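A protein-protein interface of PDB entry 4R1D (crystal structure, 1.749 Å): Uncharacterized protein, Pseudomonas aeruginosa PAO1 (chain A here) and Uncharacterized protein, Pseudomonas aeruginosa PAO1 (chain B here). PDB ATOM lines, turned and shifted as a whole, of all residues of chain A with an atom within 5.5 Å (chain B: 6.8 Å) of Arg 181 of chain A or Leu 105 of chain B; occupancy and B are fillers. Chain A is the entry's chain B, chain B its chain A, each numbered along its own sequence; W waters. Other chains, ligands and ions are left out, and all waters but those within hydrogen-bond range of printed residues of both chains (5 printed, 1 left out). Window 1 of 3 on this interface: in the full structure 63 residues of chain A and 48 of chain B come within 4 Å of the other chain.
OD2 of Asp 67 of chain B lies within salt-bridge range of NH1 of Arg 181 of chain A, at 2.8 Å. The side-chain hydroxyl (OG) of Ser 69 of chain B lies within hydrogen-bond range of the side-chain carboxylate (OE1) of Glu 179 of chain A, 2.7 Å away. The guanidinium group of Arg 97 of chain B lies within salt-bridge range of the side-chain carboxylate of Glu 179 of chain A. The guanidinium group of Arg 163 of chain A is in salt-bridge range of the side-chain carboxylate of Glu 104 of chain B. The side-chain carboxylate (OE1) of Glu 104 of chain B lies close to the side-chain hydroxyl (OG) of Ser 183 of chain A (3.4 Å). OE1 of Gln 110 of chain B lies within hydrogen-bond range of NH2 of Arg 163 of chain A (2.9 Å).
OD1 of Asp 67 of chain B lies within hydrogen-bond range of N of Ser 69 of chain B (2.9 Å). The guanidinium group (NE) of Arg 102 of chain B is in hydrogen-bond range of the backbone carbonyl oxygen (O) of Arg 97 of chain B (2.9 Å). OE2 of Glu 179 of chain A is in salt-bridge range of NE of Arg 181 of chain A, 3.0 Å away. The backbone carbonyl oxygen (O) of Arg 181 of chain A lies within hydrogen-bond range of the backbone NH (N) of Thr 258 of chain A, 2.9 Å away. The backbone carbonyl oxygen (O) of Ser 183 of chain A lies within hydrogen-bond range of the backbone NH (N) of Asn 256 of chain A, at 2.9 Å.
CB of Asp 67 of chain B touches O of Gly 165 of chain A, at 3.5 Å. C of Val 166 of chain A touches CB of Asp 67 of chain B, at 3.95 Å. Trp 96 of chain B touches Glu 179 of chain A (CZ2 to OE2, 3.7 Å). Arg 181 of chain A touches Ser 69 of chain B. Arg 97 of chain B touches Arg 181 of chain A. CD2 of Leu 105 of chain B touches NH1 of Arg 181 of chain A, 3.5 Å away. Lys 100 of chain B touches Ser 183 of chain A (CE to OG, 3.2 Å). Lys 100 of chain B touches Asn 256 of chain A. Thr 258 of chain A touches Trp 96 of chain B. O of Ala 259 of chain A touches CH2 of Trp 96 of chain B, 3.7 Å away.
Of the printed residues of chain A, Ser 69 of chain B touches Glu 179 (2.7 Å) and Arg 181 (3.6 Å). Of the printed residues of chain B, Ala 259 of chain A touches Trp 96 (3.7 Å). Arg 63 of chain B touches none of the printed residues of chain A. The nearest residue of chain B that does not touch Arg 181 of chain A is Asn 64 of chain B (4.2 Å). The nearest printed residue of chain B that does not touch Ala 259 of chain A is Arg 97 of chain B (7.5 Å).
Of the 23 printed residues of chain B, 8 touch a printed residue of chain A. Hydrophobic or aromatic side chains of chain B that line the printed part of chain A: Trp 96 and Leu 105.
Water W2 bridges NZ of Lys 107 of chain B and NH2 of Arg 163 of chain A. Water W3 lies within hydrogen-bond range of the side-chain hydroxyl of Ser 183 of chain A (2.7 Å) and the side-chain carboxylate of Glu 104 of chain B (3.5 Å). Water W4 lies within hydrogen-bond range of the side-chain amide oxygen (OE1) of Gln 110 of chain B (2.7 Å), the guanidinium group (NH1) of Arg 163 of chain A (2.9 Å), the side-chain amide nitrogen (ND2) of Asn 64 of chain B (3.0 Å) and the backbone carbonyl oxygen (O) of Glu 104 of chain B (3.1 Å). Water W1 bridges the side-chain hydroxyl (OG1) of Thr 258 of chain A (2.9 Å) and the guanidinium group (NH1) of Arg 97 of chain B (3.2 Å).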
ATOM      1  N   ARG A 163      -6.466   1.988 -24.338  1.00  0.00           N
ATOM      2  CA  ARG A 163      -6.514   0.540 -24.288  1.00  0.00           C
ATOM      3  C   ARG A 163      -5.148   0.005 -24.649  1.00  0.00           C
ATOM      4  O   ARG A 163      -4.419   0.627 -25.423  1.00  0.00           O
ATOM      5  CB  ARG A 163      -7.577   0.021 -25.286  1.00  0.00           C
ATOM      6  CG  ARG A 163      -7.510  -1.485 -25.578  1.00  0.00           C
ATOM      7  CD  ARG A 163      -8.782  -1.973 -26.281  1.00  0.00           C
ATOM      8  NE  ARG A 163      -8.978  -1.411 -27.622  1.00  0.00           N
ATOM      9  CZ  ARG A 163      -8.528  -1.978 -28.738  1.00  0.00           C
ATOM     10  NH1 ARG A 163      -7.828  -3.114 -28.683  1.00  0.00           N
ATOM     11  NH2 ARG A 163      -8.778  -1.419 -29.911  1.00  0.00           N
ATOM     12  N   PHE A 164      -4.796  -1.135 -24.068  1.00  0.00           N
ATOM     13  CA  PHE A 164      -3.642  -1.889 -24.537  1.00  0.00           C
ATOM     14  C   PHE A 164      -3.949  -3.371 -24.619  1.00  0.00           C
ATOM     15  O   PHE A 164      -4.911  -3.868 -24.031  1.00  0.00           O
ATOM     16  CB  PHE A 164      -2.399  -1.639 -23.659  1.00  0.00           C
ATOM     17  CG  PHE A 164      -2.487  -2.215 -22.261  1.00  0.00           C
ATOM     18  CD1 PHE A 164      -2.274  -3.563 -22.025  1.00  0.00           C
ATOM     19  CD2 PHE A 164      -2.762  -1.393 -21.180  1.00  0.00           C
ATOM     20  CE1 PHE A 164      -2.352  -4.088 -20.730  1.00  0.00           C
ATOM     21  CE2 PHE A 164      -2.825  -1.899 -19.883  1.00  0.00           C
ATOM     22  CZ  PHE A 164      -2.617  -3.242 -19.655  1.00  0.00           C
ATOM     23  N   GLY A 165      -3.120  -4.080 -25.366  1.00  0.00           N
ATOM     24  CA  GLY A 165      -3.157  -5.521 -25.356  1.00  0.00           C
ATOM     25  C   GLY A 165      -1.730  -5.997 -25.500  1.00  0.00           C
ATOM     26  O   GLY A 165      -0.994  -5.508 -26.358  1.00  0.00           O
ATOM     27  N   VAL A 166      -1.355  -6.952 -24.656  1.00  0.00           N
ATOM     28  CA  VAL A 166      -0.004  -7.476 -24.624  1.00  0.00           C
ATOM     29  C   VAL A 166      -0.096  -8.977 -24.702  1.00  0.00           C
ATOM     30  O   VAL A 166      -0.920  -9.580 -24.028  1.00  0.00           O
ATOM     31  CB  VAL A 166       0.730  -7.081 -23.315  1.00  0.00           C
ATOM     32  CG1 VAL A 166       2.137  -7.647 -23.315  1.00  0.00           C
ATOM     33  CG2 VAL A 166       0.756  -5.571 -23.162  1.00  0.00           C
ATOM     34  N   GLU A 179      -2.026 -13.352 -22.303  1.00  0.00           N
ATOM     35  CA  GLU A 179      -2.378 -12.005 -22.742  1.00  0.00           C
ATOM     36  C   GLU A 179      -2.972 -11.152 -21.625  1.00  0.00           C
ATOM     37  O   GLU A 179      -3.678 -11.654 -20.744  1.00  0.00           O
ATOM     38  CB  GLU A 179      -3.295 -12.012 -23.969  1.00  0.00           C
ATOM     39  CG  GLU A 179      -4.513 -12.883 -23.855  1.00  0.00           C
ATOM     40  CD  GLU A 179      -5.668 -12.356 -24.707  1.00  0.00           C
ATOM     41  OE1 GLU A 179      -5.669 -12.563 -25.949  1.00  0.00           O
ATOM     42  OE2 GLU A 179      -6.566 -11.717 -24.125  1.00  0.00           O
ATOM     43  N   PHE A 180      -2.684  -9.853 -21.700  1.00  0.00           N
ATOM     44  CA  PHE A 180      -3.044  -8.865 -20.687  1.00  0.00           C
ATOM     45  C   PHE A 180      -3.612  -7.659 -21.431  1.00  0.00           C
ATOM     46  O   PHE A 180      -2.958  -7.105 -22.312  1.00  0.00           O
ATOM     47  CB  PHE A 180      -1.765  -8.492 -19.907  1.00  0.00           C
ATOM     48  CG  PHE A 180      -1.960  -7.473 -18.807  1.00  0.00           C
ATOM     49  CD1 PHE A 180      -3.090  -7.482 -18.010  1.00  0.00           C
ATOM     50  CD2 PHE A 180      -0.974  -6.528 -18.546  1.00  0.00           C
ATOM     51  CE1 PHE A 180      -3.243  -6.552 -16.982  1.00  0.00           C
ATOM     52  CE2 PHE A 180      -1.121  -5.599 -17.525  1.00  0.00           C
ATOM     53  CZ  PHE A 180      -2.258  -5.608 -16.742  1.00  0.00           C
ATOM     54  N   ARG A 181      -4.843  -7.274 -21.109  1.00  0.00           N
ATOM     55  CA  ARG A 181      -5.492  -6.160 -21.802  1.00  0.00           C
ATOM     56  C   ARG A 181      -6.174  -5.241 -20.807  1.00  0.00           C
ATOM     57  O   ARG A 181      -6.675  -5.708 -19.781  1.00  0.00           O
ATOM     58  CB  ARG A 181      -6.578  -6.687 -22.761  1.00  0.00           C
ATOM     59  CG  ARG A 181      -6.078  -7.643 -23.822  1.00  0.00           C
ATOM     60  CD  ARG A 181      -7.162  -8.093 -24.797  1.00  0.00           C
ATOM     61  NE  ARG A 181      -6.567  -9.117 -25.646  1.00  0.00           N
ATOM     62  CZ  ARG A 181      -5.787  -8.851 -26.687  1.00  0.00           C
ATOM     63  NH1 ARG A 181      -5.568  -7.592 -27.044  1.00  0.00           N
ATOM     64  NH2 ARG A 181      -5.234  -9.846 -27.374  1.00  0.00           N
ATOM     65  N   SER A 182      -6.229  -3.949 -21.126  1.00  0.00           N
ATOM     66  CA  SER A 182      -7.082  -3.014 -20.390  1.00  0.00           C
ATOM     67  C   SER A 182      -7.817  -2.150 -21.398  1.00  0.00           C
ATOM     68  O   SER A 182      -7.277  -1.814 -22.464  1.00  0.00           O
ATOM     69  CB  SER A 182      -6.275  -2.130 -19.412  1.00  0.00           C
ATOM     70  OG  SER A 182      -5.788  -0.957 -20.044  1.00  0.00           O
ATOM     71  N   SER A 183      -9.046  -1.787 -21.058  1.00  0.00           N
ATOM     72  CA  SER A 183      -9.869  -0.993 -21.939  1.00  0.00           C
ATOM     73  C   SER A 183     -10.781  -0.130 -21.078  1.00  0.00           C
ATOM     74  O   SER A 183     -11.446  -0.639 -20.177  1.00  0.00           O
ATOM     75  CB  SER A 183     -10.706  -1.932 -22.817  1.00  0.00           C
ATOM     76  OG  SER A 183     -11.621  -1.190 -23.604  1.00  0.00           O
ATOM     77  N   ASN A 256     -11.792  -1.875 -17.605  1.00  0.00           N
ATOM     78  CA  ASN A 256     -11.927  -3.305 -17.755  1.00  0.00           C
ATOM     79  C   ASN A 256     -10.516  -3.886 -17.893  1.00  0.00           C
ATOM     80  O   ASN A 256      -9.689  -3.319 -18.604  1.00  0.00           O
ATOM     81  CB  ASN A 256     -12.755  -3.626 -18.987  1.00  0.00           C
ATOM     82  CG  ASN A 256     -12.830  -5.102 -19.254  1.00  0.00           C
ATOM     83  OD1 ASN A 256     -12.068  -5.630 -20.064  1.00  0.00           O
ATOM     84  ND2 ASN A 256     -13.738  -5.790 -18.565  1.00  0.00           N
ATOM     85  N   LEU A 257     -10.239  -4.982 -17.187  1.00  0.00           N
ATOM     86  CA  LEU A 257      -8.921  -5.608 -17.226  1.00  0.00           C
ATOM     87  C   LEU A 257      -9.076  -7.101 -17.453  1.00  0.00           C
ATOM     88  O   LEU A 257      -9.867  -7.752 -16.794  1.00  0.00           O
ATOM     89  CB  LEU A 257      -8.182  -5.381 -15.903  1.00  0.00           C
ATOM     90  CG  LEU A 257      -6.654  -5.308 -15.897  1.00  0.00           C
ATOM     91  CD1 LEU A 257      -6.196  -4.037 -16.574  1.00  0.00           C
ATOM     92  CD2 LEU A 257      -6.132  -5.355 -14.468  1.00  0.00           C
ATOM     93  N   THR A 258      -8.313  -7.651 -18.386  1.00  0.00           N
ATOM     94  CA  THR A 258      -8.348  -9.091 -18.552  1.00  0.00           C
ATOM     95  C   THR A 258      -6.931  -9.657 -18.546  1.00  0.00           C
ATOM     96  O   THR A 258      -5.974  -8.990 -18.948  1.00  0.00           O
ATOM     97  CB  THR A 258      -9.067  -9.536 -19.862  1.00  0.00           C
ATOM     98  OG1 THR A 258      -8.384  -8.990 -20.999  1.00  0.00           O
ATOM     99  CG2 THR A 258     -10.536  -9.079 -19.869  1.00  0.00           C
ATOM    100  N   ALA A 259      -6.828 -10.880 -18.057  1.00  0.00           N
ATOM    101  CA  ALA A 259      -5.611 -11.670 -18.153  1.00  0.00           C
ATOM    102  C   ALA A 259      -6.043 -13.064 -18.565  1.00  0.00           C
ATOM    103  O   ALA A 259      -7.043 -13.591 -18.068  1.00  0.00           O
ATOM    104  CB  ALA A 259      -4.875 -11.700 -16.799  1.00  0.00           C
ATOM    105  N   LEU B  62      -7.609 -15.408 -37.339  1.00  0.00           N
ATOM    106  CA  LEU B  62      -7.038 -14.073 -37.166  1.00  0.00           C
ATOM    107  C   LEU B  62      -6.399 -13.935 -35.800  1.00  0.00           C
ATOM    108  O   LEU B  62      -6.851 -14.539 -34.822  1.00  0.00           O
ATOM    109  CB  LEU B  62      -8.118 -12.987 -37.273  1.00  0.00           C
ATOM    110  CG  LEU B  62      -9.009 -13.035 -38.511  1.00  0.00           C
ATOM    111  CD1 LEU B  62     -10.120 -12.004 -38.369  1.00  0.00           C
ATOM    112  CD2 LEU B  62      -8.183 -12.794 -39.779  1.00  0.00           C
ATOM    113  N   ARG B  63      -5.363 -13.114 -35.746  1.00  0.00           N
ATOM    114  CA  ARG B  63      -4.744 -12.752 -34.490  1.00  0.00           C
ATOM    115  C   ARG B  63      -4.613 -11.245 -34.437  1.00  0.00           C
ATOM    116  O   ARG B  63      -4.628 -10.580 -35.470  1.00  0.00           O
ATOM    117  CB  ARG B  63      -3.369 -13.415 -34.371  1.00  0.00           C
ATOM    118  CG  ARG B  63      -2.385 -12.954 -35.438  1.00  0.00           C
ATOM    119  CD  ARG B  63      -1.112 -13.787 -35.391  1.00  0.00           C
ATOM    120  NE  ARG B  63      -0.147 -13.323 -36.384  1.00  0.00           N
ATOM    121  CZ  ARG B  63       0.753 -14.104 -36.969  1.00  0.00           C
ATOM    122  NH1 ARG B  63       0.792 -15.403 -36.685  1.00  0.00           N
ATOM    123  NH2 ARG B  63       1.592 -13.596 -37.855  1.00  0.00           N
ATOM    124  N   ASN B  64      -4.481 -10.701 -33.231  1.00  0.00           N
ATOM    125  CA  ASN B  64      -4.289  -9.257 -33.092  1.00  0.00           C
ATOM    126  C   ASN B  64      -2.954  -8.871 -33.737  1.00  0.00           C
ATOM    127  O   ASN B  64      -1.939  -9.517 -33.506  1.00  0.00           O
ATOM    128  CB  ASN B  64      -4.339  -8.849 -31.606  1.00  0.00           C
ATOM    129  CG  ASN B  64      -4.115  -7.354 -31.392  1.00  0.00           C
ATOM    130  OD1 ASN B  64      -2.975  -6.883 -31.411  1.00  0.00           O
ATOM    131  ND2 ASN B  64      -5.206  -6.600 -31.154  1.00  0.00           N
ATOM    132  N   ASP B  67      -0.330  -7.608 -30.893  1.00  0.00           N
ATOM    133  CA  ASP B  67       0.052  -8.470 -29.767  1.00  0.00           C
ATOM    134  C   ASP B  67       0.150  -9.947 -30.110  1.00  0.00           C
ATOM    135  O   ASP B  67       0.668 -10.736 -29.320  1.00  0.00           O
ATOM    136  CB  ASP B  67      -0.821  -8.219 -28.515  1.00  0.00           C
ATOM    137  CG  ASP B  67      -2.290  -8.586 -28.710  1.00  0.00           C
ATOM    138  OD1 ASP B  67      -2.577  -9.732 -29.088  1.00  0.00           O
ATOM    139  OD2 ASP B  67      -3.160  -7.725 -28.438  1.00  0.00           O
ATOM    140  N   LYS B  68      -0.355 -10.298 -31.295  1.00  0.00           N
ATOM    141  CA  LYS B  68      -0.255 -11.641 -31.866  1.00  0.00           C
ATOM    142  C   LYS B  68      -1.121 -12.721 -31.204  1.00  0.00           C
ATOM    143  O   LYS B  68      -1.028 -13.900 -31.568  1.00  0.00           O
ATOM    144  CB  LYS B  68       1.217 -12.099 -31.968  1.00  0.00           C
ATOM    145  CG  LYS B  68       2.166 -11.064 -32.555  1.00  0.00           C
ATOM    146  CD  LYS B  68       1.725 -10.617 -33.961  1.00  0.00           C
ATOM    147  CE  LYS B  68       2.719  -9.665 -34.583  1.00  0.00           C
ATOM    148  NZ  LYS B  68       2.235  -9.202 -35.915  1.00  0.00           N
ATOM    149  N   SER B  69      -1.971 -12.338 -30.254  1.00  0.00           N
ATOM    150  CA  SER B  69      -2.832 -13.322 -29.604  1.00  0.00           C
ATOM    151  C   SER B  69      -3.998 -13.668 -30.521  1.00  0.00           C
ATOM    152  O   SER B  69      -4.371 -12.869 -31.389  1.00  0.00           O
ATOM    153  CB  SER B  69      -3.331 -12.836 -28.238  1.00  0.00           C
ATOM    154  OG  SER B  69      -3.936 -13.909 -27.518  1.00  0.00           O
ATOM    155  N   GLU B  70      -4.549 -14.866 -30.350  1.00  0.00           N
ATOM    156  CA  GLU B  70      -5.627 -15.353 -31.218  1.00  0.00           C
ATOM    157  C   GLU B  70      -6.947 -14.642 -30.910  1.00  0.00           C
ATOM    158  O   GLU B  70      -7.372 -14.607 -29.758  1.00  0.00           O
ATOM    159  CB  GLU B  70      -5.809 -16.861 -31.026  1.00  0.00           C
ATOM    160  CG  GLU B  70      -4.617 -17.724 -31.427  1.00  0.00           C
ATOM    161  CD  GLU B  70      -3.504 -17.760 -30.385  1.00  0.00           C
ATOM    162  OE1 GLU B  70      -3.689 -17.197 -29.286  1.00  0.00           O
ATOM    163  OE2 GLU B  70      -2.443 -18.364 -30.668  1.00  0.00           O
ATOM    164  N   VAL B  71      -7.600 -14.085 -31.931  1.00  0.00           N
ATOM    165  CA  VAL B  71      -8.896 -13.439 -31.743  1.00  0.00           C
ATOM    166  C   VAL B  71      -9.999 -14.088 -32.577  1.00  0.00           C
ATOM    167  O   VAL B  71     -11.169 -13.759 -32.419  1.00  0.00           O
ATOM    168  CB  VAL B  71      -8.845 -11.934 -32.094  1.00  0.00           C
ATOM    169  CG1 VAL B  71      -7.907 -11.190 -31.135  1.00  0.00           C
ATOM    170  CG2 VAL B  71      -8.397 -11.753 -33.522  1.00  0.00           C
ATOM    171  N   THR B  93     -11.148 -17.764 -28.014  1.00  0.00           N
ATOM    172  CA  THR B  93     -11.278 -16.691 -28.991  1.00  0.00           C
ATOM    173  C   THR B  93     -12.592 -15.927 -28.862  1.00  0.00           C
ATOM    174  O   THR B  93     -12.679 -14.776 -29.285  1.00  0.00           O
ATOM    175  CB  THR B  93     -11.179 -17.209 -30.443  1.00  0.00           C
ATOM    176  OG1 THR B  93     -12.188 -18.201 -30.665  1.00  0.00           O
ATOM    177  CG2 THR B  93      -9.798 -17.788 -30.705  1.00  0.00           C
ATOM    178  N   TRP B  96     -15.268 -16.262 -23.931  1.00  0.00           N
ATOM    179  CA  TRP B  96     -14.883 -15.475 -22.748  1.00  0.00           C
ATOM    180  C   TRP B  96     -14.699 -13.992 -23.032  1.00  0.00           C
ATOM    181  O   TRP B  96     -14.448 -13.209 -22.107  1.00  0.00           O
ATOM    182  CB  TRP B  96     -13.616 -16.039 -22.073  1.00  0.00           C
ATOM    183  CG  TRP B  96     -12.285 -15.522 -22.590  1.00  0.00           C
ATOM    184  CD1 TRP B  96     -11.713 -15.788 -23.803  1.00  0.00           C
ATOM    185  CD2 TRP B  96     -11.332 -14.710 -21.873  1.00  0.00           C
ATOM    186  NE1 TRP B  96     -10.485 -15.174 -23.895  1.00  0.00           N
ATOM    187  CE2 TRP B  96     -10.225 -14.516 -22.722  1.00  0.00           C
ATOM    188  CE3 TRP B  96     -11.311 -14.132 -20.599  1.00  0.00           C
ATOM    189  CZ2 TRP B  96      -9.108 -13.758 -22.343  1.00  0.00           C
ATOM    190  CZ3 TRP B  96     -10.195 -13.377 -20.221  1.00  0.00           C
ATOM    191  CH2 TRP B  96      -9.115 -13.195 -21.094  1.00  0.00           C
ATOM    192  N   ARG B  97     -14.823 -13.615 -24.304  1.00  0.00           N
ATOM    193  CA  ARG B  97     -14.702 -12.213 -24.704  1.00  0.00           C
ATOM    194  C   ARG B  97     -16.030 -11.498 -24.508  1.00  0.00           C
ATOM    195  O   ARG B  97     -17.026 -11.876 -25.130  1.00  0.00           O
ATOM    196  CB  ARG B  97     -14.332 -12.116 -26.185  1.00  0.00           C
ATOM    197  CG  ARG B  97     -13.109 -12.938 -26.600  1.00  0.00           C
ATOM    198  CD  ARG B  97     -11.831 -12.298 -26.116  1.00  0.00           C
ATOM    199  NE  ARG B  97     -10.647 -12.919 -26.710  1.00  0.00           N
ATOM    200  CZ  ARG B  97      -9.405 -12.703 -26.282  1.00  0.00           C
ATOM    201  NH1 ARG B  97      -9.191 -11.872 -25.263  1.00  0.00           N
ATOM    202  NH2 ARG B  97      -8.376 -13.296 -26.886  1.00  0.00           N
ATOM    203  N   LYS B 100     -17.830  -5.593 -25.492  1.00  0.00           N
ATOM    204  CA  LYS B 100     -16.944  -4.494 -25.808  1.00  0.00           C
ATOM    205  C   LYS B 100     -15.606  -5.046 -26.293  1.00  0.00           C
ATOM    206  O   LYS B 100     -15.059  -4.573 -27.282  1.00  0.00           O
ATOM    207  CB  LYS B 100     -16.765  -3.564 -24.592  1.00  0.00           C
ATOM    208  CG  LYS B 100     -15.774  -2.437 -24.804  1.00  0.00           C
ATOM    209  CD  LYS B 100     -16.006  -1.298 -23.821  1.00  0.00           C
ATOM    210  CE  LYS B 100     -14.774  -1.007 -22.990  1.00  0.00           C
ATOM    211  NZ  LYS B 100     -14.601  -1.946 -21.841  1.00  0.00           N
ATOM    212  N   ALA B 101     -15.086  -6.056 -25.604  1.00  0.00           N
ATOM    213  CA  ALA B 101     -13.831  -6.672 -26.040  1.00  0.00           C
ATOM    214  C   ALA B 101     -13.949  -7.182 -27.480  1.00  0.00           C
ATOM    215  O   ALA B 101     -13.039  -6.980 -28.297  1.00  0.00           O
ATOM    216  CB  ALA B 101     -13.436  -7.803 -25.103  1.00  0.00           C
ATOM    217  N   ARG B 102     -15.071  -7.825 -27.801  1.00  0.00           N
ATOM    218  CA  ARG B 102     -15.242  -8.382 -29.148  1.00  0.00           C
ATOM    219  C   ARG B 102     -15.195  -7.302 -30.197  1.00  0.00           C
ATOM    220  O   ARG B 102     -14.611  -7.492 -31.256  1.00  0.00           O
ATOM    221  CB  ARG B 102     -16.564  -9.143 -29.288  1.00  0.00           C
ATOM    222  CG  ARG B 102     -16.612 -10.430 -28.492  1.00  0.00           C
ATOM    223  CD  ARG B 102     -18.019 -11.021 -28.527  1.00  0.00           C
ATOM    224  NE  ARG B 102     -18.069 -12.291 -27.819  1.00  0.00           N
ATOM    225  CZ  ARG B 102     -19.178 -12.997 -27.645  1.00  0.00           C
ATOM    226  NH1 ARG B 102     -20.322 -12.553 -28.139  1.00  0.00           N
ATOM    227  NH2 ARG B 102     -19.140 -14.147 -26.989  1.00  0.00           N
ATOM    228  N   GLN B 103     -15.831  -6.173 -29.902  1.00  0.00           N
ATOM    229  CA  GLN B 103     -15.857  -5.060 -30.831  1.00  0.00           C
ATOM    230  C   GLN B 103     -14.466  -4.469 -31.032  1.00  0.00           C
ATOM    231  O   GLN B 103     -14.105  -4.054 -32.129  1.00  0.00           O
ATOM    232  CB  GLN B 103     -16.812  -3.981 -30.328  1.00  0.00           C
ATOM    233  CG  GLN B 103     -16.885  -2.788 -31.240  1.00  0.00           C
ATOM    234  CD  GLN B 103     -18.013  -1.856 -30.868  1.00  0.00           C
ATOM    235  OE1 GLN B 103     -17.915  -1.115 -29.895  1.00  0.00           O
ATOM    236  NE2 GLN B 103     -19.100  -1.895 -31.641  1.00  0.00           N
ATOM    237  N   GLU B 104     -13.676  -4.443 -29.965  1.00  0.00           N
ATOM    238  CA  GLU B 104     -12.304  -3.959 -30.064  1.00  0.00           C
ATOM    239  C   GLU B 104     -11.390  -4.924 -30.794  1.00  0.00           C
ATOM    240  O   GLU B 104     -10.518  -4.506 -31.552  1.00  0.00           O
ATOM    241  CB  GLU B 104     -11.729  -3.721 -28.674  1.00  0.00           C
ATOM    242  CG  GLU B 104     -12.442  -2.660 -27.916  1.00  0.00           C
ATOM    243  CD  GLU B 104     -12.120  -2.672 -26.420  1.00  0.00           C
ATOM    244  OE1 GLU B 104     -11.519  -3.654 -25.892  1.00  0.00           O
ATOM    245  OE2 GLU B 104     -12.496  -1.681 -25.766  1.00  0.00           O
ATOM    246  N   LEU B 105     -11.555  -6.213 -30.539  1.00  0.00           N
ATOM    247  CA  LEU B 105     -10.603  -7.181 -31.072  1.00  0.00           C
ATOM    248  C   LEU B 105     -10.915  -7.623 -32.506  1.00  0.00           C
ATOM    249  O   LEU B 105     -10.017  -8.033 -33.232  1.00  0.00           O
ATOM    250  CB  LEU B 105     -10.528  -8.393 -30.156  1.00  0.00           C
ATOM    251  CG  LEU B 105     -10.027  -8.055 -28.744  1.00  0.00           C
ATOM    252  CD1 LEU B 105     -10.225  -9.224 -27.804  1.00  0.00           C
ATOM    253  CD2 LEU B 105      -8.549  -7.631 -28.794  1.00  0.00           C
ATOM    254  N   LEU B 106     -12.176  -7.552 -32.909  1.00  0.00           N
ATOM    255  CA  LEU B 106     -12.539  -7.916 -34.285  1.00  0.00           C
ATOM    256  C   LEU B 106     -12.705  -6.639 -35.100  1.00  0.00           C
ATOM    257  O   LEU B 106     -13.781  -6.336 -35.627  1.00  0.00           O
ATOM    258  CB  LEU B 106     -13.789  -8.807 -34.317  1.00  0.00           C
ATOM    259  CG  LEU B 106     -13.607 -10.184 -33.651  1.00  0.00           C
ATOM    260  CD1 LEU B 106     -14.925 -10.950 -33.556  1.00  0.00           C
ATOM    261  CD2 LEU B 106     -12.535 -11.031 -34.366  1.00  0.00           C
ATOM    262  N   LYS B 107     -11.610  -5.892 -35.171  1.00  0.00           N
ATOM    263  CA  LYS B 107     -11.540  -4.612 -35.837  1.00  0.00           C
ATOM    264  C   LYS B 107     -10.576  -4.824 -36.992  1.00  0.00           C
ATOM    265  O   LYS B 107      -9.420  -5.225 -36.786  1.00  0.00           O
ATOM    266  CB  LYS B 107     -10.995  -3.555 -34.871  1.00  0.00           C
ATOM    267  CG  LYS B 107     -11.656  -2.197 -34.974  1.00  0.00           C
ATOM    268  CD  LYS B 107     -11.391  -1.371 -33.720  1.00  0.00           C
ATOM    269  CE  LYS B 107     -12.014   0.016 -33.821  1.00  0.00           C
ATOM    270  NZ  LYS B 107     -11.915   0.790 -32.547  1.00  0.00           N
ATOM    271  N   ALA B 108     -11.064  -4.589 -38.206  1.00  0.00           N
ATOM    272  CA  ALA B 108     -10.331  -4.915 -39.420  1.00  0.00           C
ATOM    273  C   ALA B 108      -8.878  -4.445 -39.418  1.00  0.00           C
ATOM    274  O   ALA B 108      -7.973  -5.215 -39.754  1.00  0.00           O
ATOM    275  CB  ALA B 108     -11.065  -4.376 -40.643  1.00  0.00           C
ATOM    276  N   GLN B 110      -6.891  -3.871 -37.128  1.00  0.00           N
ATOM    277  CA  GLN B 110      -6.130  -4.285 -35.960  1.00  0.00           C
ATOM    278  C   GLN B 110      -5.948  -5.799 -35.867  1.00  0.00           C
ATOM    279  O   GLN B 110      -5.492  -6.310 -34.844  1.00  0.00           O
ATOM    280  CB  GLN B 110      -6.771  -3.730 -34.687  1.00  0.00           C
ATOM    281  CG  GLN B 110      -6.747  -2.191 -34.672  1.00  0.00           C
ATOM    282  CD  GLN B 110      -7.472  -1.583 -33.491  1.00  0.00           C
ATOM    283  OE1 GLN B 110      -7.859  -2.278 -32.557  1.00  0.00           O
ATOM    284  NE2 GLN B 110      -7.689  -0.274 -33.549  1.00  0.00           N
ATOM    285  N   VAL B 111      -6.294  -6.509 -36.944  1.00  0.00           N
ATOM    286  CA  VAL B 111      -6.096  -7.950 -37.004  1.00  0.00           C
ATOM    287  C   VAL B 111      -5.278  -8.340 -38.229  1.00  0.00           C
ATOM    288  O   VAL B 111      -5.123  -7.554 -39.145  1.00  0.00           O
ATOM    289  CB  VAL B 111      -7.445  -8.732 -37.056  1.00  0.00           C
ATOM    290  CG1 VAL B 111      -8.285  -8.467 -35.797  1.00  0.00           C
ATOM    291  CG2 VAL B 111      -8.227  -8.415 -38.349  1.00  0.00           C
ATOM    292  N   LEU B 212     -12.531  -9.269 -42.226  1.00  0.00           N
ATOM    293  CA  LEU B 212     -13.155  -8.072 -41.655  1.00  0.00           C
ATOM    294  C   LEU B 212     -12.972  -6.840 -42.537  1.00  0.00           C
ATOM    295  O   LEU B 212     -13.807  -5.925 -42.548  1.00  0.00           O
ATOM    296  CB  LEU B 212     -12.585  -7.793 -40.264  1.00  0.00           C
ATOM    297  CG  LEU B 212     -13.061  -8.780 -39.200  1.00  0.00           C
ATOM    298  CD1 LEU B 212     -12.148  -8.713 -37.992  1.00  0.00           C
ATOM    299  CD2 LEU B 212     -14.510  -8.426 -38.808  1.00  0.00           C
HETATM  300  O   HOH W   1     -10.136  -9.565 -23.232  1.00  0.00           O
HETATM  301  O   HOH W   2     -11.249  -0.164 -30.284  1.00  0.00           O
HETATM  302  O   HOH W   3     -11.113   1.261 -24.586  1.00  0.00           O
HETATM  303  O   HOH W   4      -7.448  -4.558 -31.146  1.00  0.00           O
HETATM  304  O   HOH W   5     -14.114  -4.523 -22.112  1.00  0.00           O
